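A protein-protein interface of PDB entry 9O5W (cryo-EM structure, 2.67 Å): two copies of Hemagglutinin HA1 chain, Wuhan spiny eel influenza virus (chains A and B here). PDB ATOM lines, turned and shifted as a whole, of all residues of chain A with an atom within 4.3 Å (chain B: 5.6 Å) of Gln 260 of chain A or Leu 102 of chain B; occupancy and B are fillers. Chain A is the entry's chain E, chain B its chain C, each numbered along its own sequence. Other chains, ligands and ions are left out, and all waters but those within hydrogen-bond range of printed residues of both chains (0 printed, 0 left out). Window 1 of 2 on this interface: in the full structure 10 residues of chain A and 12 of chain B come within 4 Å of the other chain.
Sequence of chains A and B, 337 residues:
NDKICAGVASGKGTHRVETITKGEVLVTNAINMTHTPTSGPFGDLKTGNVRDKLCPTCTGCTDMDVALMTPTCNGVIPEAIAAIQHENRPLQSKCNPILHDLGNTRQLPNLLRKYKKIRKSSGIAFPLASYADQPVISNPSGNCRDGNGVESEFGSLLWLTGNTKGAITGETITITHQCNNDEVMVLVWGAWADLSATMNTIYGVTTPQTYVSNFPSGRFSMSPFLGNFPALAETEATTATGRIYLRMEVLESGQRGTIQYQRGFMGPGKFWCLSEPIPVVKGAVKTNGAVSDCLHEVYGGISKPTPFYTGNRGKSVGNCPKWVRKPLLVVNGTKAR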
ATOM      1  N   GLU A 171     -24.377  16.220   9.142  1.00  0.00           N
ATOM      2  CA  GLU A 171     -25.179  16.666  10.270  1.00  0.00           C
ATOM      3  C   GLU A 171     -24.374  17.705  11.031  1.00  0.00           C
ATOM      4  O   GLU A 171     -23.149  17.712  10.967  1.00  0.00           O
ATOM      5  CB  GLU A 171     -25.533  15.495  11.189  1.00  0.00           C
ATOM      6  CG  GLU A 171     -26.340  14.399  10.511  1.00  0.00           C
ATOM      7  CD  GLU A 171     -27.752  14.819  10.185  1.00  0.00           C
ATOM      8  OE1 GLU A 171     -28.194  15.874  10.684  1.00  0.00           O
ATOM      9  OE2 GLU A 171     -28.427  14.094   9.423  1.00  0.00           O
ATOM     10  N   THR A 172     -25.064  18.597  11.738  1.00  0.00           N
ATOM     11  CA  THR A 172     -24.414  19.649  12.510  1.00  0.00           C
ATOM     12  C   THR A 172     -24.926  19.604  13.939  1.00  0.00           C
ATOM     13  O   THR A 172     -26.138  19.510  14.159  1.00  0.00           O
ATOM     14  CB  THR A 172     -24.686  21.028  11.887  1.00  0.00           C
ATOM     15  OG1 THR A 172     -24.244  21.033  10.524  1.00  0.00           O
ATOM     16  CG2 THR A 172     -23.949  22.140  12.639  1.00  0.00           C
ATOM     17  N   TYR A 211     -15.188  15.515   8.259  1.00  0.00           N
ATOM     18  CA  TYR A 211     -15.501  15.960   9.608  1.00  0.00           C
ATOM     19  C   TYR A 211     -14.940  17.363   9.760  1.00  0.00           C
ATOM     20  O   TYR A 211     -13.820  17.637   9.322  1.00  0.00           O
ATOM     21  CB  TYR A 211     -14.896  15.037  10.659  1.00  0.00           C
ATOM     22  CG  TYR A 211     -15.323  13.608  10.487  1.00  0.00           C
ATOM     23  CD1 TYR A 211     -14.597  12.755   9.672  1.00  0.00           C
ATOM     24  CD2 TYR A 211     -16.451  13.110  11.118  1.00  0.00           C
ATOM     25  CE1 TYR A 211     -14.964  11.455   9.504  1.00  0.00           C
ATOM     26  CE2 TYR A 211     -16.831  11.801  10.947  1.00  0.00           C
ATOM     27  CZ  TYR A 211     -16.084  10.984  10.130  1.00  0.00           C
ATOM     28  OH  TYR A 211     -16.428   9.678   9.938  1.00  0.00           O
ATOM     29  N   VAL A 212     -15.717  18.243  10.379  1.00  0.00           N
ATOM     30  CA  VAL A 212     -15.356  19.641  10.573  1.00  0.00           C
ATOM     31  C   VAL A 212     -15.741  20.032  11.989  1.00  0.00           C
ATOM     32  O   VAL A 212     -16.762  19.574  12.512  1.00  0.00           O
ATOM     33  CB  VAL A 212     -16.039  20.562   9.534  1.00  0.00           C
ATOM     34  CG1 VAL A 212     -15.673  22.028   9.752  1.00  0.00           C
ATOM     35  CG2 VAL A 212     -15.686  20.141   8.117  1.00  0.00           C
ATOM     36  N   ASN A 214     -15.506  23.748  14.672  1.00  0.00           N
ATOM     37  CA  ASN A 214     -15.177  25.161  14.821  1.00  0.00           C
ATOM     38  C   ASN A 214     -15.368  25.544  16.278  1.00  0.00           C
ATOM     39  O   ASN A 214     -16.504  25.588  16.767  1.00  0.00           O
ATOM     40  CB  ASN A 214     -16.047  26.034  13.920  1.00  0.00           C
ATOM     41  CG  ASN A 214     -15.585  27.472  13.895  1.00  0.00           C
ATOM     42  OD1 ASN A 214     -14.436  27.760  13.573  1.00  0.00           O
ATOM     43  ND2 ASN A 214     -16.476  28.385  14.257  1.00  0.00           N
ATOM     44  N   ARG A 219     -10.849  26.581  13.308  1.00  0.00           N
ATOM     45  CA  ARG A 219     -11.485  25.565  12.484  1.00  0.00           C
ATOM     46  C   ARG A 219     -10.553  24.374  12.299  1.00  0.00           C
ATOM     47  O   ARG A 219      -9.346  24.535  12.103  1.00  0.00           O
ATOM     48  CB  ARG A 219     -11.860  26.137  11.116  1.00  0.00           C
ATOM     49  CG  ARG A 219     -12.623  25.179  10.209  1.00  0.00           C
ATOM     50  CD  ARG A 219     -13.001  25.871   8.920  1.00  0.00           C
ATOM     51  NE  ARG A 219     -13.671  25.000   7.959  1.00  0.00           N
ATOM     52  CZ  ARG A 219     -14.982  24.800   7.883  1.00  0.00           C
ATOM     53  NH1 ARG A 219     -15.830  25.394   8.708  1.00  0.00           N
ATOM     54  NH2 ARG A 219     -15.458  23.994   6.939  1.00  0.00           N
ATOM     55  N   THR A 258     -19.072  24.176  17.237  1.00  0.00           N
ATOM     56  CA  THR A 258     -19.888  23.457  16.259  1.00  0.00           C
ATOM     57  C   THR A 258     -19.116  22.266  15.709  1.00  0.00           C
ATOM     58  O   THR A 258     -17.923  22.384  15.436  1.00  0.00           O
ATOM     59  CB  THR A 258     -20.313  24.383  15.110  1.00  0.00           C
ATOM     60  OG1 THR A 258     -21.093  25.463  15.634  1.00  0.00           O
ATOM     61  CG2 THR A 258     -21.161  23.635  14.072  1.00  0.00           C
ATOM     62  N   ILE A 259     -19.775  21.108  15.593  1.00  0.00           N
ATOM     63  CA  ILE A 259     -19.182  19.931  14.948  1.00  0.00           C
ATOM     64  C   ILE A 259     -20.098  19.504  13.802  1.00  0.00           C
ATOM     65  O   ILE A 259     -21.234  19.068  14.035  1.00  0.00           O
ATOM     66  CB  ILE A 259     -18.947  18.771  15.930  1.00  0.00           C
ATOM     67  CG1 ILE A 259     -18.029  19.220  17.078  1.00  0.00           C
ATOM     68  CG2 ILE A 259     -18.311  17.561  15.202  1.00  0.00           C
ATOM     69  CD1 ILE A 259     -17.922  18.240  18.229  1.00  0.00           C
ATOM     70  N   GLN A 260     -19.637  19.712  12.568  1.00  0.00           N
ATOM     71  CA  GLN A 260     -20.258  19.161  11.367  1.00  0.00           C
ATOM     72  C   GLN A 260     -19.645  17.797  11.058  1.00  0.00           C
ATOM     73  O   GLN A 260     -18.421  17.664  11.043  1.00  0.00           O
ATOM     74  CB  GLN A 260     -20.102  20.104  10.177  1.00  0.00           C
ATOM     75  CG  GLN A 260     -20.882  21.386  10.311  1.00  0.00           C
ATOM     76  CD  GLN A 260     -21.092  22.072   8.983  1.00  0.00           C
ATOM     77  OE1 GLN A 260     -20.171  22.179   8.175  1.00  0.00           O
ATOM     78  NE2 GLN A 260     -22.314  22.525   8.741  1.00  0.00           N
ATOM     79  N   TYR A 261     -20.477  16.778  10.847  1.00  0.00           N
ATOM     80  CA  TYR A 261     -19.964  15.419  10.730  1.00  0.00           C
ATOM     81  C   TYR A 261     -20.793  14.596   9.750  1.00  0.00           C
ATOM     82  O   TYR A 261     -22.017  14.721   9.713  1.00  0.00           O
ATOM     83  CB  TYR A 261     -19.944  14.776  12.129  1.00  0.00           C
ATOM     84  CG  TYR A 261     -21.308  14.443  12.738  1.00  0.00           C
ATOM     85  CD1 TYR A 261     -22.027  13.315  12.348  1.00  0.00           C
ATOM     86  CD2 TYR A 261     -21.843  15.232  13.744  1.00  0.00           C
ATOM     87  CE1 TYR A 261     -23.233  13.007  12.913  1.00  0.00           C
ATOM     88  CE2 TYR A 261     -23.059  14.929  14.314  1.00  0.00           C
ATOM     89  CZ  TYR A 261     -23.750  13.820  13.886  1.00  0.00           C
ATOM     90  OH  TYR A 261     -24.967  13.501  14.430  1.00  0.00           O
ATOM     91  N   LEU B  99     -23.751  31.790   8.861  1.00  0.00           N
ATOM     92  CA  LEU B  99     -23.379  30.805   9.871  1.00  0.00           C
ATOM     93  C   LEU B  99     -22.123  31.287  10.590  1.00  0.00           C
ATOM     94  O   LEU B  99     -21.005  30.829  10.351  1.00  0.00           O
ATOM     95  CB  LEU B  99     -23.192  29.438   9.230  1.00  0.00           C
ATOM     96  CG  LEU B  99     -24.434  28.853   8.552  1.00  0.00           C
ATOM     97  CD1 LEU B  99     -24.067  27.589   7.822  1.00  0.00           C
ATOM     98  CD2 LEU B  99     -25.563  28.571   9.538  1.00  0.00           C
ATOM     99  N   HIS B 100     -22.333  32.239  11.500  1.00  0.00           N
ATOM    100  CA  HIS B 100     -21.231  32.924  12.162  1.00  0.00           C
ATOM    101  C   HIS B 100     -20.488  32.017  13.132  1.00  0.00           C
ATOM    102  O   HIS B 100     -19.333  32.304  13.461  1.00  0.00           O
ATOM    103  CB  HIS B 100     -21.752  34.141  12.926  1.00  0.00           C
ATOM    104  CG  HIS B 100     -22.227  35.260  12.055  1.00  0.00           C
ATOM    105  ND1 HIS B 100     -21.376  36.022  11.287  1.00  0.00           N
ATOM    106  CD2 HIS B 100     -23.467  35.760  11.847  1.00  0.00           C
ATOM    107  CE1 HIS B 100     -22.070  36.934  10.633  1.00  0.00           C
ATOM    108  NE2 HIS B 100     -23.342  36.800  10.959  1.00  0.00           N
ATOM    109  N   ASP B 101     -21.116  30.935  13.590  1.00  0.00           N
ATOM    110  CA  ASP B 101     -20.504  29.995  14.519  1.00  0.00           C
ATOM    111  C   ASP B 101     -19.779  28.856  13.812  1.00  0.00           C
ATOM    112  O   ASP B 101     -19.303  27.933  14.480  1.00  0.00           O
ATOM    113  CB  ASP B 101     -21.566  29.424  15.459  1.00  0.00           C
ATOM    114  CG  ASP B 101     -22.068  30.444  16.450  1.00  0.00           C
ATOM    115  OD1 ASP B 101     -21.232  31.136  17.068  1.00  0.00           O
ATOM    116  OD2 ASP B 101     -23.300  30.559  16.613  1.00  0.00           O
ATOM    117  N   LEU B 102     -19.677  28.912  12.482  1.00  0.00           N
ATOM    118  CA  LEU B 102     -18.968  27.924  11.679  1.00  0.00           C
ATOM    119  C   LEU B 102     -17.765  28.569  10.994  1.00  0.00           C
ATOM    120  O   LEU B 102     -17.287  28.084   9.965  1.00  0.00           O
ATOM    121  CB  LEU B 102     -19.922  27.292  10.660  1.00  0.00           C
ATOM    122  CG  LEU B 102     -20.808  26.148  11.168  1.00  0.00           C
ATOM    123  CD1 LEU B 102     -21.987  26.649  11.997  1.00  0.00           C
ATOM    124  CD2 LEU B 102     -21.304  25.304  10.011  1.00  0.00           C
ATOM    125  N   GLY B 103     -17.257  29.645  11.579  1.00  0.00           N
ATOM    126  CA  GLY B 103     -16.136  30.374  11.034  1.00  0.00           C
ATOM    127  C   GLY B 103     -15.607  31.301  12.101  1.00  0.00           C
ATOM    128  O   GLY B 103     -15.902  31.127  13.284  1.00  0.00           O
ATOM    129  N   ASN B 104     -14.836  32.306  11.680  1.00  0.00           N
ATOM    130  CA  ASN B 104     -14.202  33.230  12.616  1.00  0.00           C
ATOM    131  C   ASN B 104     -14.787  34.635  12.534  1.00  0.00           C
ATOM    132  O   ASN B 104     -14.153  35.589  12.993  1.00  0.00           O
ATOM    133  CB  ASN B 104     -12.700  33.291  12.352  1.00  0.00           C
ATOM    134  CG  ASN B 104     -12.373  33.885  10.999  1.00  0.00           C
ATOM    135  OD1 ASN B 104     -13.173  33.811  10.070  1.00  0.00           O
ATOM    136  ND2 ASN B 104     -11.189  34.467  10.878  1.00  0.00           N
ATOM    137  N   PHE B 225     -21.269  22.025   3.282  1.00  0.00           N
ATOM    138  CA  PHE B 225     -22.220  20.970   2.974  1.00  0.00           C
ATOM    139  C   PHE B 225     -23.460  21.613   2.365  1.00  0.00           C
ATOM    140  O   PHE B 225     -23.852  22.720   2.741  1.00  0.00           O
ATOM    141  CB  PHE B 225     -22.597  20.179   4.228  1.00  0.00           C
ATOM    142  CG  PHE B 225     -21.480  19.330   4.783  1.00  0.00           C
ATOM    143  CD1 PHE B 225     -20.827  18.402   3.994  1.00  0.00           C
ATOM    144  CD2 PHE B 225     -21.101  19.452   6.107  1.00  0.00           C
ATOM    145  CE1 PHE B 225     -19.805  17.633   4.509  1.00  0.00           C
ATOM    146  CE2 PHE B 225     -20.081  18.681   6.624  1.00  0.00           C
ATOM    147  CZ  PHE B 225     -19.438  17.768   5.827  1.00  0.00           C
ATOM    148  N   PRO B 230     -28.574  24.404   9.654  1.00  0.00           N
ATOM    149  CA  PRO B 230     -29.124  24.758  10.967  1.00  0.00           C
ATOM    150  C   PRO B 230     -30.359  25.632  10.824  1.00  0.00           C
ATOM    151  O   PRO B 230     -30.552  26.298   9.805  1.00  0.00           O
ATOM    152  CB  PRO B 230     -27.977  25.513  11.645  1.00  0.00           C
ATOM    153  CG  PRO B 230     -26.766  25.011  10.999  1.00  0.00           C
ATOM    154  CD  PRO B 230     -27.138  24.740   9.580  1.00  0.00           C
ATOM    155  N   TYR B 245     -21.525  31.058   4.358  1.00  0.00           N
ATOM    156  CA  TYR B 245     -20.341  30.726   5.145  1.00  0.00           C
ATOM    157  C   TYR B 245     -19.339  31.860   4.959  1.00  0.00           C
ATOM    158  O   TYR B 245     -18.911  32.099   3.830  1.00  0.00           O
ATOM    159  CB  TYR B 245     -19.737  29.405   4.677  1.00  0.00           C
ATOM    160  CG  TYR B 245     -20.511  28.174   5.080  1.00  0.00           C
ATOM    161  CD1 TYR B 245     -21.675  27.819   4.415  1.00  0.00           C
ATOM    162  CD2 TYR B 245     -20.048  27.334   6.080  1.00  0.00           C
ATOM    163  CE1 TYR B 245     -22.388  26.696   4.774  1.00  0.00           C
ATOM    164  CE2 TYR B 245     -20.751  26.204   6.443  1.00  0.00           C
ATOM    165  CZ  TYR B 245     -21.916  25.887   5.782  1.00  0.00           C
ATOM    166  OH  TYR B 245     -22.607  24.750   6.122  1.00  0.00           O
ATOM    167  N   LEU B 246     -18.945  32.544   6.035  1.00  0.00           N
ATOM    168  CA  LEU B 246     -17.982  33.640   5.923  1.00  0.00           C
ATOM    169  C   LEU B 246     -16.645  33.377   6.595  1.00  0.00           C
ATOM    170  O   LEU B 246     -16.533  32.613   7.558  1.00  0.00           O
ATOM    171  CB  LEU B 246     -18.494  34.953   6.496  1.00  0.00           C
ATOM    172  CG  LEU B 246     -19.690  35.690   5.948  1.00  0.00           C
ATOM    173  CD1 LEU B 246     -19.866  36.927   6.801  1.00  0.00           C
ATOM    174  CD2 LEU B 246     -19.458  36.041   4.516  1.00  0.00           C
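Asn 214 of chain A touches Leu 102 of chain B (ND2 to C, 3.5 Å). Leu 102 of chain B touches Thr 258 of chain A. Leu 102 of chain B touches Gln 260 of chain A. Gln 260 of chain A touches Phe 225 of chain B.
O of Gln 260 of chain A lies within hydrogen-bond range of N of Val 212 of chain A. OG1 of Thr 172 of chain A lies within hydrogen-bond range of NE2 of Gln 260 of chain A. N of Asn 214 of chain A lies within hydrogen-bond range of O of Thr 258 of chain A (2.9 Å).
Of chain A, only Asn 214 (3.5 Å), Arg 219 (3.3 Å), Thr 258 (3.8 Å) and Gln 260 (3.2 Å) come within 4 Å of Leu 102 of chain B. Of the printed residues of chain B, Thr 258 of chain A touches Asp 101 and Leu 102. Of the printed residues of chain B, Arg 219 of chain A touches Leu 102 (3.3 Å). The nearest residue of chain B that does not touch Gln 260 of chain A is Pro 230 of chain B (5.4 Å). The nearest printed residue of chain A that does not touch Gly 103 of chain B is Arg 219 of chain A (5.3 Å).
Printed residues of chain A that touch a printed residue of chain B: Asn 214, Arg 219, Thr 258 and Gln 260. Hydrophobic or aromatic side chains of chain B that line the printed part of chain A: Leu 102, Phe 225 and Tyr 245. Among the printed residues, no Asp or Glu carboxylate lies within 4 Å of a Lys or Arg side-chain nitrogen of the other chain.
No position is printed for both chains.
The side-chain hydroxyl (OH) of Tyr 245 of chain B sits at hydrogen-bond distance from the side-chain amide nitrogen (NE2) of Gln 260 of chain A (3.4 Å). The backbone carbonyl oxygen of Gly 103 of chain B is in hydrogen-bond range of the side-chain amide nitrogen of Asn 214 of chain A (3.0 Å). O of Leu 102 of chain B lies within hydrogen-bond range of NH1 of Arg 219 of chain A, 3.3 Å away. O of Asp 101 of chain B sits at hydrogen-bond distance from ND2 of Asn 214 of chain A, at 2.9 Å. The backbone carbonyl oxygen (O) of Asp 101 of chain B lies within hydrogen-bond range of the side-chain hydroxyl (OG1) of Thr 258 of chain A (3.3 Å).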
